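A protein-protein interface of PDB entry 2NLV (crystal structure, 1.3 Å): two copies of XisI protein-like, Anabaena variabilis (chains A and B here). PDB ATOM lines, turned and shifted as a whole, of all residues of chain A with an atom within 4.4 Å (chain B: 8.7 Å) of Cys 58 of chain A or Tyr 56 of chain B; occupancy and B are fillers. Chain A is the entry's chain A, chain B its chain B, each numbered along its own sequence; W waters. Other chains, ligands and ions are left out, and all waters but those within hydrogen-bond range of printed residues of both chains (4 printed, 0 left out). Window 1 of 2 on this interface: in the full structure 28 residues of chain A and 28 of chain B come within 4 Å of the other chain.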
ATOM      1  N   GLN A  43       2.252 -24.057  17.700  1.00  0.00           N
ATOM      2  CA  GLN A  43       3.384 -23.994  18.619  1.00  0.00           C
ATOM      3  C   GLN A  43       3.118 -23.072  19.808  1.00  0.00           C
ATOM      4  O   GLN A  43       2.401 -22.077  19.694  1.00  0.00           O
ATOM      5  CB  GLN A  43       4.666 -23.465  17.924  1.00  0.00           C
ATOM      6  CG  GLN A  43       5.128 -24.248  16.718  1.00  0.00           C
ATOM      7  CD  GLN A  43       6.483 -23.774  16.164  1.00  0.00           C
ATOM      8  OE1 GLN A  43       6.964 -24.309  15.151  1.00  0.00           O
ATOM      9  NE2 GLN A  43       7.112 -22.807  16.830  1.00  0.00           N
ATOM     10  N   TRP A  44       3.762 -23.376  20.922  1.00  0.00           N
ATOM     11  CA  TRP A  44       3.992 -22.435  21.998  1.00  0.00           C
ATOM     12  C   TRP A  44       5.483 -22.244  22.125  1.00  0.00           C
ATOM     13  O   TRP A  44       6.214 -23.185  22.361  1.00  0.00           O
ATOM     14  CB  TRP A  44       3.419 -22.922  23.286  1.00  0.00           C
ATOM     15  CG  TRP A  44       3.970 -22.106  24.493  1.00  0.00           C
ATOM     16  CD1 TRP A  44       4.435 -20.804  24.484  1.00  0.00           C
ATOM     17  CD2 TRP A  44       4.145 -22.576  25.790  1.00  0.00           C
ATOM     18  NE1 TRP A  44       4.898 -20.457  25.733  1.00  0.00           N
ATOM     19  CE2 TRP A  44       4.703 -21.535  26.560  1.00  0.00           C
ATOM     20  CE3 TRP A  44       3.857 -23.762  26.393  1.00  0.00           C
ATOM     21  CZ2 TRP A  44       5.008 -21.689  27.921  1.00  0.00           C
ATOM     22  CZ3 TRP A  44       4.170 -23.902  27.785  1.00  0.00           C
ATOM     23  CH2 TRP A  44       4.734 -22.907  28.486  1.00  0.00           C
ATOM     24  N   MET A  45       5.929 -21.032  21.886  1.00  0.00           N
ATOM     25  CA  MET A  45       7.353 -20.640  22.025  1.00  0.00           C
ATOM     26  C   MET A  45       7.606 -19.586  23.069  1.00  0.00           C
ATOM     27  O   MET A  45       6.709 -18.790  23.446  1.00  0.00           O
ATOM     28  CB  MET A  45       7.949 -20.084  20.726  1.00  0.00           C
ATOM     29  CG  MET A  45       8.006 -21.036  19.555  1.00  0.00           C
ATOM     30  SD  MET A  45       9.200 -20.344  18.233  1.00  0.00           S
ATOM     31  CE  MET A  45      10.846 -20.619  19.223  1.00  0.00           C
ATOM     32  N   ARG A  57      12.884 -20.753  22.044  1.00  0.00           N
ATOM     33  CA  ARG A  57      12.623 -22.154  22.252  1.00  0.00           C
ATOM     34  C   ARG A  57      11.178 -22.453  22.085  1.00  0.00           C
ATOM     35  O   ARG A  57      10.326 -21.676  22.444  1.00  0.00           O
ATOM     36  CB  ARG A  57      13.088 -22.572  23.629  1.00  0.00           C
ATOM     37  CG  ARG A  57      12.473 -21.790  24.710  1.00  0.00           C
ATOM     38  CD  ARG A  57      13.220 -21.986  26.011  1.00  0.00           C
ATOM     39  NE  ARG A  57      12.970 -23.307  26.578  1.00  0.00           N
ATOM     40  CZ  ARG A  57      11.992 -23.605  27.447  1.00  0.00           C
ATOM     41  NH1 ARG A  57      11.101 -22.702  27.856  1.00  0.00           N
ATOM     42  NH2 ARG A  57      11.882 -24.846  27.897  1.00  0.00           N
ATOM     43  N   CYS A  58      10.938 -23.599  21.514  1.00  0.00           N
ATOM     44  CA  CYS A  58       9.621 -24.115  21.358  1.00  0.00           C
ATOM     45  C   CYS A  58       9.345 -25.100  22.474  1.00  0.00           C
ATOM     46  O   CYS A  58      10.037 -26.095  22.577  1.00  0.00           O
ATOM     47  CB  CYS A  58       9.450 -24.759  20.001  1.00  0.00           C
ATOM     48  SG  CYS A  58       7.728 -25.399  19.830  1.00  0.00           S
ATOM     49  N   VAL A  59       8.357 -24.787  23.305  1.00  0.00           N
ATOM     50  CA  VAL A  59       8.029 -25.628  24.438  1.00  0.00           C
ATOM     51  C   VAL A  59       7.181 -26.838  24.028  1.00  0.00           C
ATOM     52  O   VAL A  59       7.447 -27.921  24.423  1.00  0.00           O
ATOM     53  CB  VAL A  59       7.349 -24.850  25.550  1.00  0.00           C
ATOM     54  CG1 VAL A  59       7.132 -25.778  26.772  1.00  0.00           C
ATOM     55  CG2 VAL A  59       8.190 -23.578  25.893  1.00  0.00           C
ATOM     56  N   ILE A  60       6.143 -26.614  23.236  1.00  0.00           N
ATOM     57  CA  ILE A  60       5.376 -27.698  22.608  1.00  0.00           C
ATOM     58  C   ILE A  60       5.022 -27.319  21.191  1.00  0.00           C
ATOM     59  O   ILE A  60       4.776 -26.162  20.866  1.00  0.00           O
ATOM     60  CB  ILE A  60       4.064 -28.031  23.326  1.00  0.00           C
ATOM     61  CG1 ILE A  60       4.311 -28.404  24.780  1.00  0.00           C
ATOM     62  CG2 ILE A  60       3.337 -29.188  22.579  1.00  0.00           C
ATOM     63  CD1 ILE A  60       3.060 -28.686  25.554  1.00  0.00           C
ATOM     64  N   HIS A  61       4.980 -28.343  20.352  1.00  0.00           N
ATOM     65  CA  HIS A  61       4.578 -28.182  18.945  1.00  0.00           C
ATOM     66  C   HIS A  61       3.702 -29.372  18.567  1.00  0.00           C
ATOM     67  O   HIS A  61       4.102 -30.527  18.747  1.00  0.00           O
ATOM     68  CB  HIS A  61       5.838 -28.144  18.101  1.00  0.00           C
ATOM     69  CG  HIS A  61       5.658 -28.027  16.616  1.00  0.00           C
ATOM     70  ND1 HIS A  61       6.689 -27.596  15.825  1.00  0.00           N
ATOM     71  CD2 HIS A  61       4.628 -28.294  15.764  1.00  0.00           C
ATOM     72  CE1 HIS A  61       6.314 -27.578  14.553  1.00  0.00           C
ATOM     73  NE2 HIS A  61       5.073 -28.016  14.478  1.00  0.00           N
ATOM     74  N   GLN A  72       5.391 -33.019  18.154  1.00  0.00           N
ATOM     75  CA  GLN A  72       6.718 -32.835  17.609  1.00  0.00           C
ATOM     76  C   GLN A  72       7.754 -32.368  18.579  1.00  0.00           C
ATOM     77  O   GLN A  72       8.932 -32.535  18.343  1.00  0.00           O
ATOM     78  CB  GLN A  72       6.703 -31.845  16.428  1.00  0.00           C
ATOM     79  CG  GLN A  72       5.710 -32.217  15.291  1.00  0.00           C
ATOM     80  CD  GLN A  72       6.233 -33.216  14.302  1.00  0.00           C
ATOM     81  OE1 GLN A  72       7.070 -34.044  14.623  1.00  0.00           O
ATOM     82  NE2 GLN A  72       5.690 -33.171  13.073  1.00  0.00           N
ATOM     83  N   GLN A  73       7.323 -31.760  19.675  1.00  0.00           N
ATOM     84  CA  GLN A  73       8.243 -31.225  20.679  1.00  0.00           C
ATOM     85  C   GLN A  73       7.472 -31.118  21.971  1.00  0.00           C
ATOM     86  O   GLN A  73       6.301 -30.727  21.981  1.00  0.00           O
ATOM     87  CB  GLN A  73       8.710 -29.833  20.241  1.00  0.00           C
ATOM     88  CG  GLN A  73       9.514 -28.990  21.237  1.00  0.00           C
ATOM     89  CD  GLN A  73      10.935 -29.170  21.052  1.00  0.00           C
ATOM     90  OE1 GLN A  73      11.409 -30.256  20.744  1.00  0.00           O
ATOM     91  NE2 GLN A  73      11.669 -28.073  21.253  1.00  0.00           N
ATOM     92  N   LEU A  75       8.915 -29.893  25.829  1.00  0.00           N
ATOM     93  CA  LEU A  75       9.938 -29.617  26.872  1.00  0.00           C
ATOM     94  C   LEU A  75       9.370 -29.576  28.252  1.00  0.00           C
ATOM     95  O   LEU A  75      10.100 -29.275  29.194  1.00  0.00           O
ATOM     96  CB  LEU A  75      10.655 -28.299  26.545  1.00  0.00           C
ATOM     97  CG  LEU A  75      11.266 -28.176  25.165  1.00  0.00           C
ATOM     98  CD1 LEU A  75      12.084 -26.853  24.926  1.00  0.00           C
ATOM     99  CD2 LEU A  75      12.112 -29.392  24.872  1.00  0.00           C
ATOM    100  N   VAL B  29      12.727 -35.465   6.477  1.00  0.00           N
ATOM    101  CA  VAL B  29      12.628 -34.178   7.122  1.00  0.00           C
ATOM    102  C   VAL B  29      11.557 -33.338   6.412  1.00  0.00           C
ATOM    103  O   VAL B  29      11.642 -33.056   5.242  1.00  0.00           O
ATOM    104  CB  VAL B  29      13.981 -33.474   7.070  1.00  0.00           C
ATOM    105  CG1 VAL B  29      13.841 -32.002   7.549  1.00  0.00           C
ATOM    106  CG2 VAL B  29      15.066 -34.225   7.899  1.00  0.00           C
ATOM    107  N   GLU B  30      10.530 -32.991   7.141  1.00  0.00           N
ATOM    108  CA  GLU B  30       9.467 -32.154   6.642  1.00  0.00           C
ATOM    109  C   GLU B  30       9.920 -30.690   6.647  1.00  0.00           C
ATOM    110  O   GLU B  30      10.378 -30.175   7.649  1.00  0.00           O
ATOM    111  CB  GLU B  30       8.168 -32.294   7.467  1.00  0.00           C
ATOM    112  CG  GLU B  30       6.981 -31.554   6.829  1.00  0.00           C
ATOM    113  CD  GLU B  30       5.706 -31.529   7.661  1.00  0.00           C
ATOM    114  OE1 GLU B  30       5.696 -31.966   8.839  1.00  0.00           O
ATOM    115  OE2 GLU B  30       4.679 -31.035   7.085  1.00  0.00           O
ATOM    116  N   GLN B  32       8.426 -27.180   6.795  1.00  0.00           N
ATOM    117  CA  GLN B  32       7.148 -26.557   7.175  1.00  0.00           C
ATOM    118  C   GLN B  32       7.205 -25.060   6.962  1.00  0.00           C
ATOM    119  O   GLN B  32       8.206 -24.380   7.232  1.00  0.00           O
ATOM    120  CB  GLN B  32       6.801 -26.818   8.640  1.00  0.00           C
ATOM    121  CG  GLN B  32       6.798 -28.283   9.060  1.00  0.00           C
ATOM    122  CD  GLN B  32       6.404 -28.486  10.486  1.00  0.00           C
ATOM    123  OE1 GLN B  32       6.384 -27.560  11.278  1.00  0.00           O
ATOM    124  NE2 GLN B  32       6.013 -29.722  10.806  1.00  0.00           N
ATOM    125  N   ILE B  34       4.945 -21.910   8.238  1.00  0.00           N
ATOM    126  CA  ILE B  34       3.998 -21.638   9.324  1.00  0.00           C
ATOM    127  C   ILE B  34       3.683 -20.161   9.228  1.00  0.00           C
ATOM    128  O   ILE B  34       4.527 -19.292   9.424  1.00  0.00           O
ATOM    129  CB  ILE B  34       4.606 -22.010  10.674  1.00  0.00           C
ATOM    130  CG1 ILE B  34       5.099 -23.477  10.698  1.00  0.00           C
ATOM    131  CG2 ILE B  34       3.565 -21.748  11.772  1.00  0.00           C
ATOM    132  CD1 ILE B  34       5.629 -23.965  12.033  1.00  0.00           C
ATOM    133  N   GLN B  43       7.173 -18.579  10.093  1.00  0.00           N
ATOM    134  CA  GLN B  43       8.342 -19.426  10.246  1.00  0.00           C
ATOM    135  C   GLN B  43       8.539 -20.371   9.063  1.00  0.00           C
ATOM    136  O   GLN B  43       7.578 -20.793   8.406  1.00  0.00           O
ATOM    137  CB  GLN B  43       8.211 -20.308  11.484  1.00  0.00           C
ATOM    138  CG  GLN B  43       8.136 -19.591  12.808  1.00  0.00           C
ATOM    139  CD  GLN B  43       7.786 -20.515  13.887  1.00  0.00           C
ATOM    140  OE1 GLN B  43       8.562 -20.695  14.878  1.00  0.00           O
ATOM    141  NE2 GLN B  43       6.631 -21.116  13.792  1.00  0.00           N
ATOM    142  N   TRP B  44       9.797 -20.709   8.811  1.00  0.00           N
ATOM    143  CA  TRP B  44      10.208 -21.802   7.950  1.00  0.00           C
ATOM    144  C   TRP B  44      10.956 -22.799   8.826  1.00  0.00           C
ATOM    145  O   TRP B  44      11.925 -22.409   9.469  1.00  0.00           O
ATOM    146  CB  TRP B  44      11.120 -21.232   6.835  1.00  0.00           C
ATOM    147  CG  TRP B  44      11.985 -22.211   6.070  1.00  0.00           C
ATOM    148  CD1 TRP B  44      11.735 -23.514   5.718  1.00  0.00           C
ATOM    149  CD2 TRP B  44      13.271 -21.898   5.559  1.00  0.00           C
ATOM    150  NE1 TRP B  44      12.806 -24.025   5.021  1.00  0.00           N
ATOM    151  CE2 TRP B  44      13.763 -23.039   4.933  1.00  0.00           C
ATOM    152  CE3 TRP B  44      14.043 -20.760   5.592  1.00  0.00           C
ATOM    153  CZ2 TRP B  44      15.009 -23.064   4.339  1.00  0.00           C
ATOM    154  CZ3 TRP B  44      15.263 -20.787   5.023  1.00  0.00           C
ATOM    155  CH2 TRP B  44      15.747 -21.928   4.404  1.00  0.00           C
ATOM    156  N   MET B  45      10.507 -24.034   8.907  1.00  0.00           N
ATOM    157  CA  MET B  45      11.145 -24.985   9.789  1.00  0.00           C
ATOM    158  C   MET B  45      11.566 -26.254   9.039  1.00  0.00           C
ATOM    159  O   MET B  45      11.151 -26.487   7.882  1.00  0.00           O
ATOM    160  CB  MET B  45      10.197 -25.330  10.961  1.00  0.00           C
ATOM    161  CG  MET B  45       9.812 -24.116  11.873  1.00  0.00           C
ATOM    162  SD  MET B  45       9.027 -24.725  13.512  1.00  0.00           S
ATOM    163  CE  MET B  45      10.595 -25.639  14.174  1.00  0.00           C
ATOM    164  N   ASN B  46      12.390 -27.060   9.700  1.00  0.00           N
ATOM    165  CA  ASN B  46      12.700 -28.398   9.276  1.00  0.00           C
ATOM    166  C   ASN B  46      12.394 -29.300  10.480  1.00  0.00           C
ATOM    167  O   ASN B  46      12.928 -29.073  11.584  1.00  0.00           O
ATOM    168  CB  ASN B  46      14.187 -28.593   8.913  1.00  0.00           C
ATOM    169  CG  ASN B  46      14.635 -27.927   7.642  1.00  0.00           C
ATOM    170  OD1 ASN B  46      15.847 -27.867   7.461  1.00  0.00           O
ATOM    171  ND2 ASN B  46      13.766 -27.426   6.785  1.00  0.00           N
ATOM    172  N   VAL B  47      11.589 -30.348  10.279  1.00  0.00           N
ATOM    173  CA  VAL B  47      11.103 -31.222  11.356  1.00  0.00           C
ATOM    174  C   VAL B  47      11.121 -32.658  10.880  1.00  0.00           C
ATOM    175  O   VAL B  47      10.364 -33.032   9.988  1.00  0.00           O
ATOM    176  CB  VAL B  47       9.682 -30.839  11.777  1.00  0.00           C
ATOM    177  CG1 VAL B  47       9.121 -31.744  12.881  1.00  0.00           C
ATOM    178  CG2 VAL B  47       9.606 -29.334  12.218  1.00  0.00           C
ATOM    179  N   GLY B  48      11.984 -33.481  11.475  1.00  0.00           N
ATOM    180  CA  GLY B  48      12.053 -34.886  11.093  1.00  0.00           C
ATOM    181  C   GLY B  48      13.216 -35.578  11.729  1.00  0.00           C
ATOM    182  O   GLY B  48      13.534 -35.306  12.874  1.00  0.00           O
ATOM    183  N   TRP B  49      13.813 -36.511  10.999  1.00  0.00           N
ATOM    184  CA  TRP B  49      14.861 -37.382  11.514  1.00  0.00           C
ATOM    185  C   TRP B  49      15.908 -37.626  10.471  1.00  0.00           C
ATOM    186  O   TRP B  49      15.598 -37.662   9.293  1.00  0.00           O
ATOM    187  CB  TRP B  49      14.269 -38.734  11.961  1.00  0.00           C
ATOM    188  CG  TRP B  49      13.424 -38.580  13.166  1.00  0.00           C
ATOM    189  CD1 TRP B  49      12.107 -38.181  13.220  1.00  0.00           C
ATOM    190  CD2 TRP B  49      13.856 -38.738  14.502  1.00  0.00           C
ATOM    191  NE1 TRP B  49      11.730 -38.099  14.512  1.00  0.00           N
ATOM    192  CE2 TRP B  49      12.772 -38.419  15.333  1.00  0.00           C
ATOM    193  CE3 TRP B  49      15.045 -39.149  15.099  1.00  0.00           C
ATOM    194  CZ2 TRP B  49      12.845 -38.509  16.719  1.00  0.00           C
ATOM    195  CZ3 TRP B  49      15.107 -39.207  16.492  1.00  0.00           C
ATOM    196  CH2 TRP B  49      14.018 -38.911  17.270  1.00  0.00           C
ATOM    197  N   GLN B  50      17.155 -37.732  10.871  1.00  0.00           N
ATOM    198  CA  GLN B  50      18.178 -38.304   9.989  1.00  0.00           C
ATOM    199  C   GLN B  50      18.806 -39.379  10.853  1.00  0.00           C
ATOM    200  O   GLN B  50      19.444 -39.082  11.851  1.00  0.00           O
ATOM    201  CB  GLN B  50      19.183 -37.264   9.497  1.00  0.00           C
ATOM    202  CG  GLN B  50      18.557 -36.015   8.878  1.00  0.00           C
ATOM    203  CD  GLN B  50      18.145 -36.079   7.377  1.00  0.00           C
ATOM    204  OE1 GLN B  50      18.629 -35.212   6.580  1.00  0.00           O
ATOM    205  NE2 GLN B  50      17.180 -36.999   7.002  1.00  0.00           N
ATOM    206  N   ASN B  53      19.063 -39.192  14.751  1.00  0.00           N
ATOM    207  CA  ASN B  53      19.174 -37.786  15.108  1.00  0.00           C
ATOM    208  C   ASN B  53      17.883 -37.047  14.865  1.00  0.00           C
ATOM    209  O   ASN B  53      17.424 -36.996  13.727  1.00  0.00           O
ATOM    210  CB  ASN B  53      20.269 -37.111  14.273  1.00  0.00           C
ATOM    211  CG  ASN B  53      21.622 -37.684  14.533  1.00  0.00           C
ATOM    212  OD1 ASN B  53      22.050 -37.735  15.694  1.00  0.00           O
ATOM    213  ND2 ASN B  53      22.265 -38.215  13.479  1.00  0.00           N
ATOM    214  N   ARG B  54      17.337 -36.410  15.877  1.00  0.00           N
ATOM    215  CA  ARG B  54      16.136 -35.588  15.717  1.00  0.00           C
ATOM    216  C   ARG B  54      16.513 -34.294  15.020  1.00  0.00           C
ATOM    217  O   ARG B  54      17.383 -33.576  15.495  1.00  0.00           O
ATOM    218  CB  ARG B  54      15.509 -35.298  17.063  1.00  0.00           C
ATOM    219  CG  ARG B  54      14.315 -34.315  17.032  1.00  0.00           C
ATOM    220  CD  ARG B  54      13.234 -34.761  16.137  1.00  0.00           C
ATOM    221  NE  ARG B  54      11.974 -34.067  16.378  1.00  0.00           N
ATOM    222  CZ  ARG B  54      10.951 -34.230  15.575  1.00  0.00           C
ATOM    223  NH1 ARG B  54      11.111 -34.842  14.423  1.00  0.00           N
ATOM    224  NH2 ARG B  54       9.771 -33.737  15.916  1.00  0.00           N
ATOM    225  N   ILE B  55      15.814 -33.971  13.954  1.00  0.00           N
ATOM    226  CA  ILE B  55      15.972 -32.678  13.255  1.00  0.00           C
ATOM    227  C   ILE B  55      14.755 -31.851  13.662  1.00  0.00           C
ATOM    228  O   ILE B  55      13.585 -32.211  13.375  1.00  0.00           O
ATOM    229  CB  ILE B  55      16.025 -32.821  11.747  1.00  0.00           C
ATOM    230  CG1 ILE B  55      17.127 -33.807  11.303  1.00  0.00           C
ATOM    231  CG2 ILE B  55      16.079 -31.392  11.067  1.00  0.00           C
ATOM    232  CD1 ILE B  55      18.479 -33.380  11.745  1.00  0.00           C
ATOM    233  N   TYR B  56      14.980 -30.762  14.375  1.00  0.00           N
ATOM    234  CA  TYR B  56      13.900 -29.906  14.815  1.00  0.00           C
ATOM    235  C   TYR B  56      14.479 -28.509  14.909  1.00  0.00           C
ATOM    236  O   TYR B  56      15.162 -28.163  15.871  1.00  0.00           O
ATOM    237  CB  TYR B  56      13.273 -30.351  16.148  1.00  0.00           C
ATOM    238  CG  TYR B  56      12.098 -29.514  16.497  1.00  0.00           C
ATOM    239  CD1 TYR B  56      10.852 -29.802  15.972  1.00  0.00           C
ATOM    240  CD2 TYR B  56      12.237 -28.379  17.276  1.00  0.00           C
ATOM    241  CE1 TYR B  56       9.782 -28.992  16.218  1.00  0.00           C
ATOM    242  CE2 TYR B  56      11.145 -27.547  17.541  1.00  0.00           C
ATOM    243  CZ  TYR B  56       9.944 -27.846  16.952  1.00  0.00           C
ATOM    244  OH  TYR B  56       8.908 -26.932  17.187  1.00  0.00           O
ATOM    245  N   ARG B  57      14.224 -27.691  13.904  1.00  0.00           N
ATOM    246  CA  ARG B  57      14.888 -26.385  13.811  1.00  0.00           C
ATOM    247  C   ARG B  57      14.039 -25.396  13.056  1.00  0.00           C
ATOM    248  O   ARG B  57      13.557 -25.754  11.949  1.00  0.00           O
ATOM    249  CB  ARG B  57      16.262 -26.510  13.143  1.00  0.00           C
ATOM    250  CG  ARG B  57      16.278 -27.071  11.754  1.00  0.00           C
ATOM    251  CD  ARG B  57      17.705 -27.123  11.213  1.00  0.00           C
ATOM    252  NE  ARG B  57      17.677 -26.903   9.777  1.00  0.00           N
ATOM    253  CZ  ARG B  57      18.413 -26.022   9.099  1.00  0.00           C
ATOM    254  NH1 ARG B  57      19.350 -25.242   9.655  1.00  0.00           N
ATOM    255  NH2 ARG B  57      18.234 -25.948   7.804  1.00  0.00           N
ATOM    256  N   CYS B  58      13.880 -24.171  13.602  1.00  0.00           N
ATOM    257  CA  CYS B  58      13.342 -23.072  12.836  1.00  0.00           C
ATOM    258  C   CYS B  58      14.477 -22.384  12.125  1.00  0.00           C
ATOM    259  O   CYS B  58      15.411 -21.928  12.750  1.00  0.00           O
ATOM    260  CB  CYS B  58      12.567 -22.094  13.702  1.00  0.00           C
ATOM    261  SG  CYS B  58      11.976 -20.656  12.815  1.00  0.00           S
ATOM    262  N   VAL B  59      14.363 -22.348  10.803  1.00  0.00           N
ATOM    263  CA  VAL B  59      15.447 -21.795  10.001  1.00  0.00           C
ATOM    264  C   VAL B  59      15.358 -20.287   9.924  1.00  0.00           C
ATOM    265  O   VAL B  59      16.374 -19.588  10.087  1.00  0.00           O
ATOM    266  CB  VAL B  59      15.528 -22.435   8.591  1.00  0.00           C
ATOM    267  CG1 VAL B  59      16.770 -21.979   7.896  1.00  0.00           C
ATOM    268  CG2 VAL B  59      15.413 -24.006   8.666  1.00  0.00           C
ATOM    269  N   HIS B  61      12.572 -17.076  11.248  1.00  0.00           N
ATOM    270  CA  HIS B  61      11.370 -16.649  11.927  1.00  0.00           C
ATOM    271  C   HIS B  61      11.230 -15.147  11.811  1.00  0.00           C
ATOM    272  O   HIS B  61      12.175 -14.432  12.201  1.00  0.00           O
ATOM    273  CB  HIS B  61      11.493 -17.065  13.396  1.00  0.00           C
ATOM    274  CG  HIS B  61      10.298 -16.780  14.290  1.00  0.00           C
ATOM    275  ND1 HIS B  61      10.040 -17.580  15.379  1.00  0.00           N
ATOM    276  CD2 HIS B  61       9.377 -15.769  14.343  1.00  0.00           C
ATOM    277  CE1 HIS B  61       8.990 -17.098  16.039  1.00  0.00           C
ATOM    278  NE2 HIS B  61       8.569 -15.998  15.445  1.00  0.00           N
ATOM    279  N   GLN B  73      15.120 -15.252  14.070  1.00  0.00           N
ATOM    280  CA  GLN B  73      15.948 -16.423  13.912  1.00  0.00           C
ATOM    281  C   GLN B  73      16.373 -16.416  12.457  1.00  0.00           C
ATOM    282  O   GLN B  73      15.568 -16.195  11.559  1.00  0.00           O
ATOM    283  CB  GLN B  73      15.176 -17.682  14.239  1.00  0.00           C
ATOM    284  CG  GLN B  73      15.831 -19.017  13.951  1.00  0.00           C
ATOM    285  CD  GLN B  73      16.620 -19.584  15.068  1.00  0.00           C
ATOM    286  OE1 GLN B  73      17.299 -18.858  15.745  1.00  0.00           O
ATOM    287  NE2 GLN B  73      16.655 -20.905  15.181  1.00  0.00           N
ATOM    288  N   LEU B  75      19.116 -19.189  10.586  1.00  0.00           N
ATOM    289  CA  LEU B  75      20.128 -20.259  10.559  1.00  0.00           C
ATOM    290  C   LEU B  75      20.814 -20.355   9.213  1.00  0.00           C
ATOM    291  O   LEU B  75      21.739 -21.175   9.050  1.00  0.00           O
ATOM    292  CB  LEU B  75      19.537 -21.588  10.925  1.00  0.00           C
ATOM    293  CG  LEU B  75      18.975 -21.611  12.356  1.00  0.00           C
ATOM    294  CD1 LEU B  75      18.547 -23.055  12.637  1.00  0.00           C
ATOM    295  CD2 LEU B  75      19.944 -21.026  13.384  1.00  0.00           C
HETATM  296  O   HOH W   1       8.754 -35.376  12.859  1.00  0.00           O
HETATM  297  O   HOH W   2       6.524 -34.044  10.361  1.00  0.00           O
HETATM  298  O   HOH W   3       9.731 -24.069  16.810  1.00  0.00           O
HETATM  299  O   HOH W   4      11.665 -32.660  18.916  1.00  0.00           O
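OH of Tyr 56 of chain B lies within hydrogen-bond range of SG of Cys 58 of chain A (3.3 Å).
The side-chain hydroxyl (OH) of Tyr 56 of chain B is in hydrogen-bond range of a ring nitrogen (ND1) of His 61 of chain A, at 2.7 Å.
OE1 of Gln 32 of chain B lies close to NE2 of His 61 of chain A (3.5 Å).
The side-chain sulfur of Met 45 of chain B sits close to the side-chain amide oxygen of Gln 43 of chain A.
The side-chain amide oxygen (OE1) of Gln 43 of chain B lies close to the side-chain sulfur (SD) of Met 45 of chain A (3.4 Å).
The side-chain amide nitrogen of Gln 43 of chain A sits at hydrogen-bond distance from the side-chain amide oxygen of Gln 43 of chain B, at 3.2 Å.
The guanidinium group (NH2) of Arg 54 of chain B is in hydrogen-bond range of the backbone carbonyl oxygen (O) of Gln 72 of chain A, at 2.8 Å.
The backbone carbonyl oxygen (O) of Gln 32 of chain B sits at hydrogen-bond distance from the backbone NH (N) of Met 45 of chain B, at 2.9 Å.
SD of Met 45 of chain A sits close to NE2 of Gln 43 of chain A (3.5 Å).
The side-chain amide nitrogen of Gln 32 of chain B is in hydrogen-bond range of the side-chain carboxylate of Glu 30 of chain B (3.0 Å).
The side-chain sulfur (SG) of Cys 58 of chain A sits at hydrogen-bond distance from the backbone carbonyl oxygen (O) of Ile 60 of chain A (3.2 Å).
NE2 of Gln 73 of chain A is in hydrogen-bond range of O of Cys 58 of chain A (2.9 Å).
Gln 43 of chain A touches Ile 34 of chain B (OE1 to CD1, 3.4 Å).
Gln 43 of chain A touches Tyr 56 of chain B (OE1 to OH, 3.8 Å).
His 61 of chain B touches Met 45 of chain A (CE1 to SD, 3.9 Å).
Gln 72 of chain A touches Val 47 of chain B (CD to CG1, 3.5 Å).
Gln 73 of chain A touches Tyr 56 of chain B.
Of chain B, only Tyr 56 comes within 4 Å of Cys 58 of chain A.
Of the printed residues of chain A, Tyr 56 of chain B touches Gln 43 (3.8 Å), Cys 58 (3.3 Å), His 61 (2.7 Å) and Gln 73 (3.8 Å).
Of the printed residues of chain A, Gln 43 of chain B touches Gln 43 (3.2 Å) and Met 45 (3.4 Å).
Of the printed residues of chain A, Gln 32 of chain B touches His 61.
Of the printed residues of chain A, Met 45 of chain B touches Gln 43.
Of the printed residues of chain B, Gln 73 of chain A touches Tyr 56 (3.8 Å).
Of the printed residues of chain B, Met 45 of chain A touches Gln 43 and His 61.
The nearest printed residue of chain A that does not touch Tyr 56 of chain B is Gln 72 of chain A (4.1 Å).
The nearest printed residue of chain A that does not touch Arg 54 of chain B is Gln 73 of chain A (4.9 Å).
Of the 22 printed residues of chain B, 8 touch a printed residue of chain A.
Hydrophobic or aromatic side chains of chain B within 4 Å of the printed part of chain A: Ile 34, Met 45, Val 47, Tyr 56 and His 61.
Hydrophobic or aromatic side chains of chain A within 4 Å of the printed part of chain B: Met 45 and His 61.
Gln 43 of chain A touches its own counterpart, Gln 43 of chain B.
Gln 43 of chain A touches Met 45 of chain B, and with the chains exchanged Met 45 of chain A touches Gln 43 of chain B.
Met 45 of chain A touches His 61 of chain B, but with the chains exchanged His 61 of chain A does not touch Met 45 of chain B (4.1 Å).
Positions printed for both chains: 43, 44, 45, 57, 58, 59, 61, 73 and 75.
Water W1 bridges the side-chain amide oxygen (OE1) of Gln 72 of chain A (2.8 Å) and the guanidinium group (NH1) of Arg 54 of chain B (2.9 Å).
Water W4 lies within hydrogen-bond range of O of Gln 72 of chain A (2.8 Å), NE of Arg 54 of chain B (2.9 Å) and OE1 of Gln 73 of chain A (3.0 Å).
Water W3 lies within hydrogen-bond range of NE2 of Gln 43 of chain A (2.9 Å), OH of Tyr 56 of chain B (3.0 Å) and SD of Met 45 of chain B (3.4 Å).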
